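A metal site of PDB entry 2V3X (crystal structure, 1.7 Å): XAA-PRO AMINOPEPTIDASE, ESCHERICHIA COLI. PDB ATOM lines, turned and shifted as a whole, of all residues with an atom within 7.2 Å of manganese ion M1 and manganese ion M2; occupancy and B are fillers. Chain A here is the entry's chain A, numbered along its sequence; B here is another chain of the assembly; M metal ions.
The side-chain carboxylate (OD1) of Asp 271 lies close to the side-chain hydroxyl (OH) of Tyr 229, 2.8 Å away. O of Thr 273 sits at hydrogen-bond distance from N of Glu 406. NE2 of His 354 lies close to O of Val 1 of chain B, at 3.5 Å. The side-chain hydroxyl (OH) of Tyr 229 lies close to the side-chain carboxylate (OD1) of Asp 260 (2.7 Å). The side-chain carboxylate of Asp 260 lies close to the guanidinium group of Arg 404 (2.9 Å). N of Asp 260 sits at hydrogen-bond distance from O of Ile 232 (2.9 Å). The side-chain carboxylate of Glu 383 is in salt-bridge range of the guanidinium group of Arg 404, 3.9 Å away. O of Thr 381 sits at hydrogen-bond distance from OG of Ser 353, at 2.6 Å.
Thr 381 touches manganese ion M1 (CG2 to MN, 3.8 Å). The nearest printed residue that does not touch manganese ion M1 is Pro 2 of chain B (4.4 Å).
Merely in contact with manganese ion M2: Tyr 229 and Thr 273. The nearest printed residue that does not touch manganese ion M2 is Pro 2 of chain B (4.4 Å).
The side-chain carboxylate (OD1) of Asp 271 is bound to manganese ion M2. OE1 of Glu 406 is bound to manganese ion M2. The side-chain carboxylate (OD1) of Asp 260 binds manganese ion M2, 2.2 Å away. Manganese ion M2 is bound by N of Val 1 of chain B, 2.2 Å away. Manganese ion M2 is bound by OD2 of Asp 260, at 2.5 Å.
Manganese ion M1 is bound by the side-chain carboxylate of Glu 406 (2.1 Å), a ring nitrogen (NE2) of His 354 (2.2 Å), the side-chain carboxylate of Asp 271 (2.2 Å) and the side-chain carboxylate of Glu 383 (2.3 Å).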
ATOM      1  N   TYR A 229      -2.433 -12.001 -28.091  1.00  0.00           N
ATOM      2  CA  TYR A 229      -2.964 -12.207 -26.754  1.00  0.00           C
ATOM      3  C   TYR A 229      -1.975 -11.618 -25.776  1.00  0.00           C
ATOM      4  O   TYR A 229      -0.834 -11.340 -26.144  1.00  0.00           O
ATOM      5  CB  TYR A 229      -3.200 -13.678 -26.443  1.00  0.00           C
ATOM      6  CG  TYR A 229      -2.013 -14.544 -26.656  1.00  0.00           C
ATOM      7  CD1 TYR A 229      -1.745 -15.065 -27.906  1.00  0.00           C
ATOM      8  CD2 TYR A 229      -1.120 -14.838 -25.623  1.00  0.00           C
ATOM      9  CE1 TYR A 229      -0.634 -15.842 -28.136  1.00  0.00           C
ATOM     10  CE2 TYR A 229      -0.017 -15.652 -25.832  1.00  0.00           C
ATOM     11  CZ  TYR A 229       0.227 -16.147 -27.101  1.00  0.00           C
ATOM     12  OH  TYR A 229       1.329 -16.942 -27.382  1.00  0.00           O
ATOM     13  N   ILE A 232       2.643 -13.802 -21.675  1.00  0.00           N
ATOM     14  CA  ILE A 232       2.870 -14.494 -20.387  1.00  0.00           C
ATOM     15  C   ILE A 232       4.385 -14.687 -20.234  1.00  0.00           C
ATOM     16  O   ILE A 232       5.032 -15.289 -21.094  1.00  0.00           O
ATOM     17  CB  ILE A 232       2.170 -15.875 -20.433  1.00  0.00           C
ATOM     18  CG1 ILE A 232       0.653 -15.688 -20.511  1.00  0.00           C
ATOM     19  CG2 ILE A 232       2.579 -16.770 -19.273  1.00  0.00           C
ATOM     20  CD1 ILE A 232      -0.069 -16.842 -21.181  1.00  0.00           C
ATOM     21  N   ILE A 259       7.684 -18.565 -21.304  1.00  0.00           N
ATOM     22  CA  ILE A 259       7.204 -17.437 -22.106  1.00  0.00           C
ATOM     23  C   ILE A 259       6.192 -17.961 -23.114  1.00  0.00           C
ATOM     24  O   ILE A 259       6.528 -18.795 -23.943  1.00  0.00           O
ATOM     25  CB  ILE A 259       8.324 -16.743 -22.820  1.00  0.00           C
ATOM     26  CG1 ILE A 259       9.332 -16.166 -21.819  1.00  0.00           C
ATOM     27  CG2 ILE A 259       7.782 -15.605 -23.676  1.00  0.00           C
ATOM     28  CD1 ILE A 259      10.432 -15.342 -22.485  1.00  0.00           C
ATOM     29  N   ASP A 260       4.964 -17.478 -23.018  1.00  0.00           N
ATOM     30  CA  ASP A 260       3.901 -17.806 -23.980  1.00  0.00           C
ATOM     31  C   ASP A 260       3.528 -16.475 -24.631  1.00  0.00           C
ATOM     32  O   ASP A 260       3.017 -15.561 -23.974  1.00  0.00           O
ATOM     33  CB  ASP A 260       2.726 -18.447 -23.254  1.00  0.00           C
ATOM     34  CG  ASP A 260       1.703 -19.100 -24.193  1.00  0.00           C
ATOM     35  OD1 ASP A 260       1.663 -18.768 -25.380  1.00  0.00           O
ATOM     36  OD2 ASP A 260       0.943 -19.972 -23.728  1.00  0.00           O
ATOM     37  N   ALA A 261       3.882 -16.321 -25.905  1.00  0.00           N
ATOM     38  CA  ALA A 261       3.697 -15.064 -26.612  1.00  0.00           C
ATOM     39  C   ALA A 261       3.516 -15.322 -28.079  1.00  0.00           C
ATOM     40  O   ALA A 261       4.118 -16.241 -28.649  1.00  0.00           O
ATOM     41  CB  ALA A 261       4.909 -14.113 -26.393  1.00  0.00           C
ATOM     42  N   GLY A 262       2.705 -14.477 -28.690  1.00  0.00           N
ATOM     43  CA  GLY A 262       2.413 -14.593 -30.107  1.00  0.00           C
ATOM     44  C   GLY A 262       2.047 -13.258 -30.721  1.00  0.00           C
ATOM     45  O   GLY A 262       1.430 -12.410 -30.083  1.00  0.00           O
ATOM     46  N   GLY A 270       0.171 -15.868 -34.247  1.00  0.00           N
ATOM     47  CA  GLY A 270       1.163 -16.846 -33.816  1.00  0.00           C
ATOM     48  C   GLY A 270       0.916 -17.177 -32.351  1.00  0.00           C
ATOM     49  O   GLY A 270       0.228 -16.424 -31.612  1.00  0.00           O
ATOM     50  N   ASP A 271       1.471 -18.293 -31.902  1.00  0.00           N
ATOM     51  CA  ASP A 271       1.276 -18.736 -30.520  1.00  0.00           C
ATOM     52  C   ASP A 271       2.363 -19.720 -30.167  1.00  0.00           C
ATOM     53  O   ASP A 271       2.245 -20.906 -30.430  1.00  0.00           O
ATOM     54  CB  ASP A 271      -0.128 -19.326 -30.357  1.00  0.00           C
ATOM     55  CG  ASP A 271      -0.440 -19.777 -28.948  1.00  0.00           C
ATOM     56  OD1 ASP A 271       0.347 -19.537 -28.014  1.00  0.00           O
ATOM     57  OD2 ASP A 271      -1.520 -20.361 -28.759  1.00  0.00           O
ATOM     58  N   ILE A 272       3.435 -19.230 -29.550  1.00  0.00           N
ATOM     59  CA  ILE A 272       4.568 -20.084 -29.187  1.00  0.00           C
ATOM     60  C   ILE A 272       4.773 -20.032 -27.669  1.00  0.00           C
ATOM     61  O   ILE A 272       4.646 -18.962 -27.066  1.00  0.00           O
ATOM     62  CB  ILE A 272       5.847 -19.652 -29.900  1.00  0.00           C
ATOM     63  CG1 ILE A 272       5.773 -19.885 -31.421  1.00  0.00           C
ATOM     64  CG2 ILE A 272       7.121 -20.337 -29.290  1.00  0.00           C
ATOM     65  CD1 ILE A 272       7.052 -19.416 -32.168  1.00  0.00           C
ATOM     66  N   THR A 273       5.113 -21.168 -27.072  1.00  0.00           N
ATOM     67  CA  THR A 273       5.625 -21.184 -25.702  1.00  0.00           C
ATOM     68  C   THR A 273       7.005 -21.842 -25.699  1.00  0.00           C
ATOM     69  O   THR A 273       7.224 -22.888 -26.340  1.00  0.00           O
ATOM     70  CB  THR A 273       4.723 -21.949 -24.695  1.00  0.00           C
ATOM     71  OG1 THR A 273       3.365 -21.488 -24.793  1.00  0.00           O
ATOM     72  CG2 THR A 273       5.211 -21.739 -23.230  1.00  0.00           C
ATOM     73  N   LEU A 352      -4.157 -30.400 -25.101  1.00  0.00           N
ATOM     74  CA  LEU A 352      -2.911 -30.454 -25.892  1.00  0.00           C
ATOM     75  C   LEU A 352      -2.876 -29.460 -27.048  1.00  0.00           C
ATOM     76  O   LEU A 352      -1.793 -29.005 -27.462  1.00  0.00           O
ATOM     77  CB  LEU A 352      -2.721 -31.874 -26.453  1.00  0.00           C
ATOM     78  CG  LEU A 352      -1.465 -32.185 -27.280  1.00  0.00           C
ATOM     79  CD1 LEU A 352      -0.198 -32.037 -26.387  1.00  0.00           C
ATOM     80  CD2 LEU A 352      -1.528 -33.575 -27.885  1.00  0.00           C
ATOM     81  N   SER A 353      -4.046 -29.170 -27.621  1.00  0.00           N
ATOM     82  CA  SER A 353      -4.123 -28.443 -28.882  1.00  0.00           C
ATOM     83  C   SER A 353      -5.380 -27.640 -28.985  1.00  0.00           C
ATOM     84  O   SER A 353      -6.462 -28.098 -28.595  1.00  0.00           O
ATOM     85  CB  SER A 353      -4.113 -29.444 -30.056  1.00  0.00           C
ATOM     86  OG  SER A 353      -2.862 -30.142 -30.133  1.00  0.00           O
ATOM     87  N   HIS A 354      -5.244 -26.463 -29.570  1.00  0.00           N
ATOM     88  CA  HIS A 354      -6.394 -25.673 -29.994  1.00  0.00           C
ATOM     89  C   HIS A 354      -6.198 -25.191 -31.427  1.00  0.00           C
ATOM     90  O   HIS A 354      -5.068 -25.021 -31.899  1.00  0.00           O
ATOM     91  CB  HIS A 354      -6.663 -24.474 -29.062  1.00  0.00           C
ATOM     92  CG  HIS A 354      -5.516 -23.531 -28.896  1.00  0.00           C
ATOM     93  ND1 HIS A 354      -5.232 -22.519 -29.804  1.00  0.00           N
ATOM     94  CD2 HIS A 354      -4.606 -23.430 -27.904  1.00  0.00           C
ATOM     95  CE1 HIS A 354      -4.160 -21.867 -29.381  1.00  0.00           C
ATOM     96  NE2 HIS A 354      -3.762 -22.399 -28.228  1.00  0.00           N
ATOM     97  N   TRP A 355      -7.302 -24.948 -32.117  1.00  0.00           N
ATOM     98  CA  TRP A 355      -7.248 -24.326 -33.426  1.00  0.00           C
ATOM     99  C   TRP A 355      -6.598 -22.944 -33.358  1.00  0.00           C
ATOM    100  O   TRP A 355      -6.664 -22.258 -32.336  1.00  0.00           O
ATOM    101  CB  TRP A 355      -8.645 -24.137 -34.020  1.00  0.00           C
ATOM    102  CG  TRP A 355      -9.577 -25.292 -34.008  1.00  0.00           C
ATOM    103  CD1 TRP A 355     -10.847 -25.289 -33.552  1.00  0.00           C
ATOM    104  CD2 TRP A 355      -9.351 -26.630 -34.527  1.00  0.00           C
ATOM    105  NE1 TRP A 355     -11.448 -26.509 -33.751  1.00  0.00           N
ATOM    106  CE2 TRP A 355     -10.545 -27.356 -34.325  1.00  0.00           C
ATOM    107  CE3 TRP A 355      -8.269 -27.261 -35.137  1.00  0.00           C
ATOM    108  CZ2 TRP A 355     -10.694 -28.685 -34.711  1.00  0.00           C
ATOM    109  CZ3 TRP A 355      -8.421 -28.600 -35.514  1.00  0.00           C
ATOM    110  CH2 TRP A 355      -9.623 -29.293 -35.300  1.00  0.00           C
ATOM    111  N   LEU A 356      -5.990 -22.528 -34.461  1.00  0.00           N
ATOM    112  CA  LEU A 356      -5.285 -21.248 -34.528  1.00  0.00           C
ATOM    113  C   LEU A 356      -5.690 -20.542 -35.830  1.00  0.00           C
ATOM    114  O   LEU A 356      -5.794 -21.183 -36.895  1.00  0.00           O
ATOM    115  CB  LEU A 356      -3.772 -21.502 -34.510  1.00  0.00           C
ATOM    116  CG  LEU A 356      -2.794 -20.328 -34.452  1.00  0.00           C
ATOM    117  CD1 LEU A 356      -2.898 -19.611 -33.108  1.00  0.00           C
ATOM    118  CD2 LEU A 356      -1.374 -20.839 -34.689  1.00  0.00           C
ATOM    119  N   VAL A 360      -6.508 -16.479 -31.539  1.00  0.00           N
ATOM    120  CA  VAL A 360      -5.545 -17.444 -30.977  1.00  0.00           C
ATOM    121  C   VAL A 360      -6.218 -18.740 -30.570  1.00  0.00           C
ATOM    122  O   VAL A 360      -5.702 -19.818 -30.882  1.00  0.00           O
ATOM    123  CB  VAL A 360      -4.679 -16.837 -29.832  1.00  0.00           C
ATOM    124  CG1 VAL A 360      -5.485 -16.391 -28.664  1.00  0.00           C
ATOM    125  CG2 VAL A 360      -3.583 -17.847 -29.442  1.00  0.00           C
ATOM    126  N   HIS A 361      -7.370 -18.662 -29.900  1.00  0.00           N
ATOM    127  CA  HIS A 361      -8.211 -19.841 -29.686  1.00  0.00           C
ATOM    128  C   HIS A 361      -9.272 -19.803 -30.784  1.00  0.00           C
ATOM    129  O   HIS A 361     -10.354 -19.186 -30.630  1.00  0.00           O
ATOM    130  CB  HIS A 361      -8.854 -19.842 -28.317  1.00  0.00           C
ATOM    131  CG  HIS A 361      -7.864 -19.990 -27.215  1.00  0.00           C
ATOM    132  ND1 HIS A 361      -8.182 -19.689 -25.905  1.00  0.00           N
ATOM    133  CD2 HIS A 361      -6.578 -20.386 -27.209  1.00  0.00           C
ATOM    134  CE1 HIS A 361      -7.122 -19.929 -25.140  1.00  0.00           C
ATOM    135  NE2 HIS A 361      -6.133 -20.346 -25.909  1.00  0.00           N
ATOM    136  N   THR A 381      -2.362 -25.664 -32.473  1.00  0.00           N
ATOM    137  CA  THR A 381      -1.185 -25.658 -31.614  1.00  0.00           C
ATOM    138  C   THR A 381      -0.934 -27.035 -31.038  1.00  0.00           C
ATOM    139  O   THR A 381      -1.820 -27.908 -31.022  1.00  0.00           O
ATOM    140  CB  THR A 381      -1.347 -24.662 -30.467  1.00  0.00           C
ATOM    141  OG1 THR A 381      -2.390 -25.121 -29.586  1.00  0.00           O
ATOM    142  CG2 THR A 381      -1.635 -23.245 -30.990  1.00  0.00           C
ATOM    143  N   VAL A 382       0.290 -27.240 -30.539  1.00  0.00           N
ATOM    144  CA  VAL A 382       0.655 -28.454 -29.832  1.00  0.00           C
ATOM    145  C   VAL A 382       1.405 -27.996 -28.598  1.00  0.00           C
ATOM    146  O   VAL A 382       2.490 -27.451 -28.724  1.00  0.00           O
ATOM    147  CB  VAL A 382       1.536 -29.378 -30.674  1.00  0.00           C
ATOM    148  CG1 VAL A 382       1.726 -30.754 -29.967  1.00  0.00           C
ATOM    149  CG2 VAL A 382       0.933 -29.540 -32.084  1.00  0.00           C
ATOM    150  N   GLU A 383       0.806 -28.167 -27.436  1.00  0.00           N
ATOM    151  CA  GLU A 383       1.305 -27.474 -26.231  1.00  0.00           C
ATOM    152  C   GLU A 383       1.226 -28.305 -24.959  1.00  0.00           C
ATOM    153  O   GLU A 383       0.574 -27.907 -23.991  1.00  0.00           O
ATOM    154  CB  GLU A 383       0.623 -26.115 -26.047  1.00  0.00           C
ATOM    155  CG  GLU A 383      -0.879 -26.090 -25.949  1.00  0.00           C
ATOM    156  CD  GLU A 383      -1.376 -24.643 -25.890  1.00  0.00           C
ATOM    157  OE1 GLU A 383      -0.967 -23.894 -24.986  1.00  0.00           O
ATOM    158  OE2 GLU A 383      -2.118 -24.260 -26.809  1.00  0.00           O
ATOM    159  N   ARG A 404       6.083 -25.506 -20.225  1.00  0.00           N
ATOM    160  CA  ARG A 404       5.261 -25.734 -21.401  1.00  0.00           C
ATOM    161  C   ARG A 404       6.091 -25.451 -22.634  1.00  0.00           C
ATOM    162  O   ARG A 404       6.934 -24.541 -22.652  1.00  0.00           O
ATOM    163  CB  ARG A 404       4.007 -24.829 -21.379  1.00  0.00           C
ATOM    164  CG  ARG A 404       3.126 -24.953 -22.615  1.00  0.00           C
ATOM    165  CD  ARG A 404       1.731 -24.354 -22.435  1.00  0.00           C
ATOM    166  NE  ARG A 404       1.678 -22.904 -22.255  1.00  0.00           N
ATOM    167  CZ  ARG A 404       1.493 -22.256 -21.082  1.00  0.00           C
ATOM    168  NH1 ARG A 404       1.409 -22.902 -19.927  1.00  0.00           N
ATOM    169  NH2 ARG A 404       1.398 -20.932 -21.052  1.00  0.00           N
ATOM    170  N   GLU A 406       5.426 -25.186 -26.874  1.00  0.00           N
ATOM    171  CA  GLU A 406       4.293 -25.087 -27.812  1.00  0.00           C
ATOM    172  C   GLU A 406       4.766 -24.654 -29.173  1.00  0.00           C
ATOM    173  O   GLU A 406       5.461 -23.625 -29.306  1.00  0.00           O
ATOM    174  CB  GLU A 406       3.300 -24.068 -27.275  1.00  0.00           C
ATOM    175  CG  GLU A 406       2.181 -23.675 -28.255  1.00  0.00           C
ATOM    176  CD  GLU A 406       1.183 -22.749 -27.631  1.00  0.00           C
ATOM    177  OE1 GLU A 406       1.548 -21.929 -26.746  1.00  0.00           O
ATOM    178  OE2 GLU A 406       0.003 -22.828 -28.022  1.00  0.00           O
ATOM    179  N   ASP A 407       4.323 -25.405 -30.179  1.00  0.00           N
ATOM    180  CA  ASP A 407       4.533 -25.116 -31.612  1.00  0.00           C
ATOM    181  C   ASP A 407       3.154 -24.991 -32.289  1.00  0.00           C
ATOM    182  O   ASP A 407       2.133 -25.451 -31.754  1.00  0.00           O
ATOM    183  CB  ASP A 407       5.350 -26.205 -32.291  1.00  0.00           C
ATOM    184  CG  ASP A 407       6.888 -26.039 -32.091  1.00  0.00           C
ATOM    185  OD1 ASP A 407       7.359 -24.892 -31.832  1.00  0.00           O
ATOM    186  OD2 ASP A 407       7.590 -27.063 -32.234  1.00  0.00           O
ATOM    187  N   ASP A 408       3.173 -24.308 -33.440  1.00  0.00           N
ATOM    188  CA  ASP A 408       1.996 -24.164 -34.289  1.00  0.00           C
ATOM    189  C   ASP A 408       2.224 -24.977 -35.562  1.00  0.00           C
ATOM    190  O   ASP A 408       3.287 -24.875 -36.180  1.00  0.00           O
ATOM    191  CB  ASP A 408       1.807 -22.705 -34.675  1.00  0.00           C
ATOM    192  CG  ASP A 408       1.761 -21.776 -33.469  1.00  0.00           C
ATOM    193  OD1 ASP A 408       1.318 -22.233 -32.394  1.00  0.00           O
ATOM    194  OD2 ASP A 408       2.142 -20.583 -33.625  1.00  0.00           O
ATOM    195  N   VAL B   1      -1.414 -19.005 -25.620  1.00  0.00           N
ATOM    196  CA  VAL B   1      -2.070 -19.187 -24.286  1.00  0.00           C
ATOM    197  C   VAL B   1      -2.947 -20.470 -24.260  1.00  0.00           C
ATOM    198  O   VAL B   1      -3.678 -20.714 -25.186  1.00  0.00           O
ATOM    199  CB  VAL B   1      -2.877 -17.933 -23.929  1.00  0.00           C
ATOM    200  CG1 VAL B   1      -3.873 -17.589 -25.035  1.00  0.00           C
ATOM    201  CG2 VAL B   1      -3.556 -18.083 -22.567  1.00  0.00           C
ATOM    202  N   PRO B   2      -2.865 -21.308 -23.185  1.00  0.00           N
ATOM    203  CA  PRO B   2      -3.592 -22.596 -23.162  1.00  0.00           C
ATOM    204  C   PRO B   2      -5.121 -22.540 -23.213  1.00  0.00           C
ATOM    205  O   PRO B   2      -5.732 -21.569 -22.745  1.00  0.00           O
ATOM    206  CB  PRO B   2      -3.146 -23.237 -21.845  1.00  0.00           C
ATOM    207  CG  PRO B   2      -1.868 -22.569 -21.524  1.00  0.00           C
ATOM    208  CD  PRO B   2      -2.028 -21.156 -21.981  1.00  0.00           C
ATOM    209  N   LEU B   3      -5.713 -23.605 -23.764  1.00  0.00           N
ATOM    210  CA  LEU B   3      -7.171 -23.812 -23.772  1.00  0.00           C
ATOM    211  C   LEU B   3      -7.498 -25.104 -23.008  1.00  0.00           C
ATOM    212  O   LEU B   3      -8.367 -25.141 -22.137  1.00  0.00           O
ATOM    213  CB  LEU B   3      -7.693 -23.894 -25.214  1.00  0.00           C
ATOM    214  CG  LEU B   3      -9.203 -24.022 -25.399  1.00  0.00           C
ATOM    215  CD1 LEU B   3      -9.918 -22.795 -24.865  1.00  0.00           C
ATOM    216  CD2 LEU B   3      -9.589 -24.260 -26.839  1.00  0.00           C
ATOM    217  OXT LEU B   3      -6.906 -26.148 -23.226  1.00  0.00           O
HETATM  218 MN    MN M   1      -1.802 -22.026 -27.405  1.00  0.00          MN
HETATM  219 MN    MN M   2       0.309 -20.304 -26.131  1.00  0.00          MN
